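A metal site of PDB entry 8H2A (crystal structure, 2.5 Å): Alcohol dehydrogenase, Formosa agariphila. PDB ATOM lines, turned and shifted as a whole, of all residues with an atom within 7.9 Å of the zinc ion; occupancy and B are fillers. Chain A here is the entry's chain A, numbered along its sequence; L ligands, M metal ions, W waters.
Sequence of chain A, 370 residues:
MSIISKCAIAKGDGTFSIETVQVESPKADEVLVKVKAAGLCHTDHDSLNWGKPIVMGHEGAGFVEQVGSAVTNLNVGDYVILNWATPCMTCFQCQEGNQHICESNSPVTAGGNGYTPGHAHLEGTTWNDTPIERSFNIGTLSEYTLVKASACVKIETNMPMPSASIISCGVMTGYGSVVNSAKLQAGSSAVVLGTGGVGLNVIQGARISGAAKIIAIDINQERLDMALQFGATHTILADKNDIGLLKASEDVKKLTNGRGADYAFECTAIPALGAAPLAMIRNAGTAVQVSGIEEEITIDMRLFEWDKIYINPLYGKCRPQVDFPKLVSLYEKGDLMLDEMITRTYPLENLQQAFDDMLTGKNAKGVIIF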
ATOM      1  N   GLY A  39     -15.553 -21.051  35.683  1.00  0.00           N
ATOM      2  CA  GLY A  39     -16.260 -21.502  34.516  1.00  0.00           C
ATOM      3  C   GLY A  39     -15.451 -22.510  33.762  1.00  0.00           C
ATOM      4  O   GLY A  39     -14.237 -22.579  33.902  1.00  0.00           O
ATOM      5  N   LEU A  40     -16.143 -23.284  32.934  1.00  0.00           N
ATOM      6  CA  LEU A  40     -15.538 -24.393  32.214  1.00  0.00           C
ATOM      7  C   LEU A  40     -15.594 -24.159  30.713  1.00  0.00           C
ATOM      8  O   LEU A  40     -16.661 -23.874  30.175  1.00  0.00           O
ATOM      9  CB  LEU A  40     -16.239 -25.698  32.554  1.00  0.00           C
ATOM     10  CG  LEU A  40     -15.264 -26.859  32.363  1.00  0.00           C
ATOM     11  CD1 LEU A  40     -14.158 -26.750  33.416  1.00  0.00           C
ATOM     12  CD2 LEU A  40     -15.984 -28.214  32.380  1.00  0.00           C
ATOM     13  N   CYS A  41     -14.456 -24.354  30.052  1.00  0.00           N
ATOM     14  CA  CYS A  41     -14.248 -24.142  28.622  1.00  0.00           C
ATOM     15  C   CYS A  41     -13.870 -25.458  27.931  1.00  0.00           C
ATOM     16  O   CYS A  41     -13.330 -26.376  28.561  1.00  0.00           O
ATOM     17  CB  CYS A  41     -13.140 -23.101  28.405  1.00  0.00           C
ATOM     18  SG  CYS A  41     -12.419 -23.121  26.741  1.00  0.00           S
ATOM     19  N   HIS A  42     -14.154 -25.534  26.632  1.00  0.00           N
ATOM     20  CA  HIS A  42     -13.732 -26.701  25.842  1.00  0.00           C
ATOM     21  C   HIS A  42     -12.212 -26.954  25.931  1.00  0.00           C
ATOM     22  O   HIS A  42     -11.772 -28.106  25.824  1.00  0.00           O
ATOM     23  CB  HIS A  42     -14.164 -26.545  24.379  1.00  0.00           C
ATOM     24  CG  HIS A  42     -13.933 -27.768  23.529  1.00  0.00           C
ATOM     25  ND1 HIS A  42     -12.685 -28.124  23.068  1.00  0.00           N
ATOM     26  CD2 HIS A  42     -14.799 -28.693  23.062  1.00  0.00           C
ATOM     27  CE1 HIS A  42     -12.792 -29.229  22.350  1.00  0.00           C
ATOM     28  NE2 HIS A  42     -14.060 -29.597  22.330  1.00  0.00           N
ATOM     29  N   THR A  43     -11.406 -25.913  26.118  1.00  0.00           N
ATOM     30  CA  THR A  43      -9.966 -26.111  26.283  1.00  0.00           C
ATOM     31  C   THR A  43      -9.622 -26.821  27.602  1.00  0.00           C
ATOM     32  O   THR A  43      -8.561 -27.448  27.693  1.00  0.00           O
ATOM     33  CB  THR A  43      -9.245 -24.771  26.222  1.00  0.00           C
ATOM     34  OG1 THR A  43      -9.669 -24.069  25.049  1.00  0.00           O
ATOM     35  CG2 THR A  43      -7.737 -24.978  26.178  1.00  0.00           C
ATOM     36  N   ASP A  44     -10.492 -26.734  28.605  1.00  0.00           N
ATOM     37  CA  ASP A  44     -10.237 -27.407  29.874  1.00  0.00           C
ATOM     38  C   ASP A  44     -10.293 -28.937  29.730  1.00  0.00           C
ATOM     39  O   ASP A  44      -9.505 -29.657  30.350  1.00  0.00           O
ATOM     40  CB  ASP A  44     -11.242 -26.914  30.926  1.00  0.00           C
ATOM     41  CG  ASP A  44     -10.805 -25.613  31.618  1.00  0.00           C
ATOM     42  OD1 ASP A  44      -9.576 -25.277  31.655  1.00  0.00           O
ATOM     43  OD2 ASP A  44     -11.691 -24.916  32.149  1.00  0.00           O
ATOM     44  N   HIS A  58      -9.322 -22.114  33.693  1.00  0.00           N
ATOM     45  CA  HIS A  58      -8.855 -20.812  33.244  1.00  0.00           C
ATOM     46  C   HIS A  58      -9.950 -19.757  33.200  1.00  0.00           C
ATOM     47  O   HIS A  58      -9.697 -18.655  32.698  1.00  0.00           O
ATOM     48  CB  HIS A  58      -8.153 -20.937  31.879  1.00  0.00           C
ATOM     49  CG  HIS A  58      -9.018 -21.489  30.795  1.00  0.00           C
ATOM     50  ND1 HIS A  58      -9.116 -22.840  30.543  1.00  0.00           N
ATOM     51  CD2 HIS A  58      -9.839 -20.887  29.912  1.00  0.00           C
ATOM     52  CE1 HIS A  58      -9.971 -23.049  29.559  1.00  0.00           C
ATOM     53  NE2 HIS A  58     -10.430 -21.874  29.153  1.00  0.00           N
ATOM     54  N   GLU A  59     -11.164 -20.033  33.701  1.00  0.00           N
ATOM     55  CA  GLU A  59     -12.200 -19.014  33.901  1.00  0.00           C
ATOM     56  C   GLU A  59     -12.512 -18.926  35.390  1.00  0.00           C
ATOM     57  O   GLU A  59     -12.992 -19.906  35.978  1.00  0.00           O
ATOM     58  CB  GLU A  59     -13.492 -19.349  33.115  1.00  0.00           C
ATOM     59  CG  GLU A  59     -13.305 -19.533  31.617  1.00  0.00           C
ATOM     60  CD  GLU A  59     -14.610 -19.708  30.849  1.00  0.00           C
ATOM     61  OE1 GLU A  59     -15.660 -19.908  31.476  1.00  0.00           O
ATOM     62  OE2 GLU A  59     -14.577 -19.661  29.605  1.00  0.00           O
ATOM     63  N   TRP A  84      -6.099 -14.644  31.840  1.00  0.00           N
ATOM     64  CA  TRP A  84      -4.895 -15.414  31.532  1.00  0.00           C
ATOM     65  C   TRP A  84      -4.026 -14.720  30.494  1.00  0.00           C
ATOM     66  O   TRP A  84      -3.187 -15.365  29.863  1.00  0.00           O
ATOM     67  CB  TRP A  84      -5.198 -16.849  31.083  1.00  0.00           C
ATOM     68  CG  TRP A  84      -6.243 -17.028  30.015  1.00  0.00           C
ATOM     69  CD1 TRP A  84      -7.601 -17.144  30.196  1.00  0.00           C
ATOM     70  CD2 TRP A  84      -6.028 -17.148  28.597  1.00  0.00           C
ATOM     71  NE1 TRP A  84      -8.236 -17.303  28.985  1.00  0.00           N
ATOM     72  CE2 TRP A  84      -7.298 -17.307  27.993  1.00  0.00           C
ATOM     73  CE3 TRP A  84      -4.894 -17.127  27.792  1.00  0.00           C
ATOM     74  CZ2 TRP A  84      -7.453 -17.443  26.605  1.00  0.00           C
ATOM     75  CZ3 TRP A  84      -5.054 -17.252  26.416  1.00  0.00           C
ATOM     76  CH2 TRP A  84      -6.320 -17.405  25.833  1.00  0.00           C
ATOM     77  N   PHE A 136      -3.078 -22.114  32.338  1.00  0.00           N
ATOM     78  CA  PHE A 136      -3.170 -20.735  31.855  1.00  0.00           C
ATOM     79  C   PHE A 136      -2.782 -19.747  32.952  1.00  0.00           C
ATOM     80  O   PHE A 136      -3.345 -18.650  33.046  1.00  0.00           O
ATOM     81  CB  PHE A 136      -4.570 -20.406  31.314  1.00  0.00           C
ATOM     82  CG  PHE A 136      -4.887 -21.075  30.004  1.00  0.00           C
ATOM     83  CD1 PHE A 136      -5.375 -22.383  29.995  1.00  0.00           C
ATOM     84  CD2 PHE A 136      -4.699 -20.411  28.777  1.00  0.00           C
ATOM     85  CE1 PHE A 136      -5.667 -23.015  28.803  1.00  0.00           C
ATOM     86  CE2 PHE A 136      -5.004 -21.048  27.575  1.00  0.00           C
ATOM     87  CZ  PHE A 136      -5.479 -22.351  27.576  1.00  0.00           C
ATOM     88  N   SER A 168     -13.749 -14.676  31.788  1.00  0.00           N
ATOM     89  CA  SER A 168     -12.321 -15.004  31.727  1.00  0.00           C
ATOM     90  C   SER A 168     -11.935 -15.767  30.471  1.00  0.00           C
ATOM     91  O   SER A 168     -10.746 -15.851  30.152  1.00  0.00           O
ATOM     92  CB  SER A 168     -11.913 -15.815  32.953  1.00  0.00           C
ATOM     93  OG  SER A 168     -12.118 -15.090  34.151  1.00  0.00           O
ATOM     94  N   CYS A 169     -12.883 -16.350  29.753  1.00  0.00           N
ATOM     95  CA  CYS A 169     -12.480 -16.946  28.485  1.00  0.00           C
ATOM     96  C   CYS A 169     -13.609 -16.861  27.458  1.00  0.00           C
ATOM     97  O   CYS A 169     -13.526 -16.060  26.516  1.00  0.00           O
ATOM     98  CB  CYS A 169     -12.012 -18.401  28.689  1.00  0.00           C
ATOM     99  SG  CYS A 169     -11.265 -19.244  27.214  1.00  0.00           S
ATOM    100  N   GLY A 170     -14.660 -17.673  27.661  1.00  0.00           N
ATOM    101  CA  GLY A 170     -15.725 -17.772  26.669  1.00  0.00           C
ATOM    102  C   GLY A 170     -16.251 -16.421  26.227  1.00  0.00           C
ATOM    103  O   GLY A 170     -16.339 -16.130  25.032  1.00  0.00           O
ATOM    104  N   THR A 173     -13.296 -14.226  24.313  1.00  0.00           N
ATOM    105  CA  THR A 173     -12.870 -14.618  22.978  1.00  0.00           C
ATOM    106  C   THR A 173     -14.000 -14.440  21.978  1.00  0.00           C
ATOM    107  O   THR A 173     -13.776 -13.884  20.893  1.00  0.00           O
ATOM    108  CB  THR A 173     -12.362 -16.055  22.929  1.00  0.00           C
ATOM    109  OG1 THR A 173     -13.494 -16.922  22.833  1.00  0.00           O
ATOM    110  CG2 THR A 173     -11.538 -16.397  24.173  1.00  0.00           C
ATOM    111  N   VAL A 198     -18.052 -20.417  23.299  1.00  0.00           N
ATOM    112  CA  VAL A 198     -17.537 -19.224  22.635  1.00  0.00           C
ATOM    113  C   VAL A 198     -18.534 -18.674  21.631  1.00  0.00           C
ATOM    114  O   VAL A 198     -18.824 -17.466  21.617  1.00  0.00           O
ATOM    115  CB  VAL A 198     -16.191 -19.521  21.944  1.00  0.00           C
ATOM    116  CG1 VAL A 198     -15.717 -18.261  21.202  1.00  0.00           C
ATOM    117  CG2 VAL A 198     -15.158 -19.956  22.955  1.00  0.00           C
ATOM    118  N   TYR A 315      -7.973 -15.183  22.274  1.00  0.00           N
ATOM    119  CA  TYR A 315      -8.497 -14.504  23.462  1.00  0.00           C
ATOM    120  C   TYR A 315      -9.195 -13.196  23.104  1.00  0.00           C
ATOM    121  O   TYR A 315      -9.219 -12.240  23.884  1.00  0.00           O
ATOM    122  CB  TYR A 315      -7.372 -14.324  24.496  1.00  0.00           C
ATOM    123  CG  TYR A 315      -7.771 -14.096  25.943  1.00  0.00           C
ATOM    124  CD1 TYR A 315      -8.994 -14.537  26.426  1.00  0.00           C
ATOM    125  CD2 TYR A 315      -6.852 -13.577  26.855  1.00  0.00           C
ATOM    126  CE1 TYR A 315      -9.351 -14.368  27.758  1.00  0.00           C
ATOM    127  CE2 TYR A 315      -7.189 -13.414  28.185  1.00  0.00           C
ATOM    128  CZ  TYR A 315      -8.444 -13.808  28.637  1.00  0.00           C
ATOM    129  OH  TYR A 315      -8.775 -13.657  29.965  1.00  0.00           O
ATOM    130  N   LYS A 365     -23.033 -22.702  29.201  1.00  0.00           N
ATOM    131  CA  LYS A 365     -21.754 -22.747  29.871  1.00  0.00           C
ATOM    132  C   LYS A 365     -22.037 -23.391  31.228  1.00  0.00           C
ATOM    133  O   LYS A 365     -23.162 -23.363  31.706  1.00  0.00           O
ATOM    134  CB  LYS A 365     -21.158 -21.333  29.993  1.00  0.00           C
ATOM    135  CG  LYS A 365     -19.865 -21.197  30.765  1.00  0.00           C
ATOM    136  CD  LYS A 365     -18.676 -21.711  30.014  1.00  0.00           C
ATOM    137  CE  LYS A 365     -18.218 -20.763  28.934  1.00  0.00           C
ATOM    138  NZ  LYS A 365     -16.887 -21.213  28.430  1.00  0.00           N
HETATM  139  P1  LIG L   1     -18.108 -26.202  23.025  1.00  0.00           P
HETATM  140  O1  LIG L   1     -17.991 -27.719  22.984  1.00  0.00           O
HETATM  141  O2  LIG L   1     -18.818 -25.723  24.311  1.00  0.00           O
HETATM  142  O3  LIG L   1     -19.012 -25.674  21.696  1.00  0.00           O
HETATM  143  C1  LIG L   1     -18.644 -26.220  20.449  1.00  0.00           C
HETATM  144  C2  LIG L   1     -19.861 -26.079  19.519  1.00  0.00           C
HETATM  145  O4  LIG L   1     -19.456 -26.503  18.362  1.00  0.00           O
HETATM  146  C3  LIG L   1     -21.015 -27.044  19.956  1.00  0.00           C
HETATM  147  O5  LIG L   1     -22.242 -26.410  19.957  1.00  0.00           O
HETATM  148  C4  LIG L   1     -20.936 -28.131  18.885  1.00  0.00           C
HETATM  149  O6  LIG L   1     -22.206 -28.866  18.708  1.00  0.00           O
HETATM  150  C5  LIG L   1     -20.646 -27.426  17.802  1.00  0.00           C
HETATM  151  N1  LIG L   1     -20.234 -28.265  16.704  1.00  0.00           N
HETATM  152  C6  LIG L   1     -19.442 -29.334  16.703  1.00  0.00           C
HETATM  153  N2  LIG L   1     -19.326 -29.779  15.458  1.00  0.00           N
HETATM  154  C7  LIG L   1     -20.051 -29.002  14.682  1.00  0.00           C
HETATM  155  C8  LIG L   1     -20.270 -29.018  13.339  1.00  0.00           C
HETATM  156  N3  LIG L   1     -19.814 -29.901  12.363  1.00  0.00           N
HETATM  157  N4  LIG L   1     -21.044 -28.072  12.799  1.00  0.00           N
HETATM  158  C9  LIG L   1     -21.616 -27.120  13.570  1.00  0.00           C
HETATM  159  N5  LIG L   1     -21.387 -27.092  14.884  1.00  0.00           N
HETATM  160  C10 LIG L   1     -20.606 -28.054  15.441  1.00  0.00           C
HETATM  161  O7  LIG L   1     -16.601 -25.521  22.934  1.00  0.00           O
HETATM  162  P2  LIG L   1     -16.232 -23.867  23.204  1.00  0.00           P
HETATM  163  O8  LIG L   1     -15.973 -23.632  24.695  1.00  0.00           O
HETATM  164  O9  LIG L   1     -17.368 -22.916  22.696  1.00  0.00           O
HETATM  165  O10 LIG L   1     -14.881 -23.571  22.373  1.00  0.00           O
HETATM  166  C11 LIG L   1     -14.896 -23.912  21.001  1.00  0.00           C
HETATM  167  C12 LIG L   1     -13.447 -23.884  20.453  1.00  0.00           C
HETATM  168  O11 LIG L   1     -12.894 -22.712  20.657  1.00  0.00           O
HETATM  169  C13 LIG L   1     -12.549 -24.941  21.180  1.00  0.00           C
HETATM  170  O12 LIG L   1     -11.762 -25.480  20.184  1.00  0.00           O
HETATM  171  C14 LIG L   1     -11.708 -24.108  22.141  1.00  0.00           C
HETATM  172  O13 LIG L   1     -10.444 -24.791  22.506  1.00  0.00           O
HETATM  173  C15 LIG L   1     -11.490 -23.000  21.399  1.00  0.00           C
HETATM  174  N6  LIG L   1     -11.154 -21.815  22.157  1.00  0.00           N
HETATM  175  C16 LIG L   1     -10.271 -20.921  21.642  1.00  0.00           C
HETATM  176  C17 LIG L   1      -9.933 -19.707  22.345  1.00  0.00           C
HETATM  177  C18 LIG L   1      -8.945 -18.691  21.784  1.00  0.00           C
HETATM  178  O14 LIG L   1      -8.401 -17.886  22.514  1.00  0.00           O
HETATM  179  N7  LIG L   1      -8.641 -18.676  20.335  1.00  0.00           N
HETATM  180  C19 LIG L   1     -10.513 -19.483  23.507  1.00  0.00           C
HETATM  181  C20 LIG L   1     -11.408 -20.381  24.012  1.00  0.00           C
HETATM  182  C21 LIG L   1     -11.744 -21.584  23.301  1.00  0.00           C
HETATM  183 ZN    ZN M   1     -10.769 -21.483  26.953  1.00  0.00          ZN
HETATM  184  O   HOH W   1      -9.258 -21.348  25.739  1.00  0.00           O
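The backbone NH (N) of Val 198 lies within hydrogen-bond range of an oxygen (O9) of the ligand, at 2.7 Å. N of His 42 sits at hydrogen-bond distance from O8 of the ligand, at 3.3 Å. An oxygen (O13) of the ligand lies within hydrogen-bond range of the side-chain hydroxyl (OG1) of Thr 43 (2.8 Å). An oxygen (O14) of the ligand is in hydrogen-bond range of the backbone NH (N) of Tyr 315, 2.7 Å away.
The zinc ion is bound by water W1 (1.9 Å), a ring nitrogen (NE2) of His 58 (2.3 Å), the side-chain sulfur of Cys 169 (2.3 Å) and the side-chain sulfur of Cys 41 (2.3 Å). The zinc ion has four donor atoms within binding distance.
Thr 43 touches the zinc ion. Four residues have an atom within 4 Å of the zinc ion: Cys 41, Thr 43, His 58 and Cys 169. The nearest printed residue that does not touch the zinc ion is Glu 59 (5.0 Å).
ND1 of His 58 sits at hydrogen-bond distance from OD1 of Asp 44, 2.7 Å away. N of Thr 43 lies close to SG of Cys 41, 3.0 Å away.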
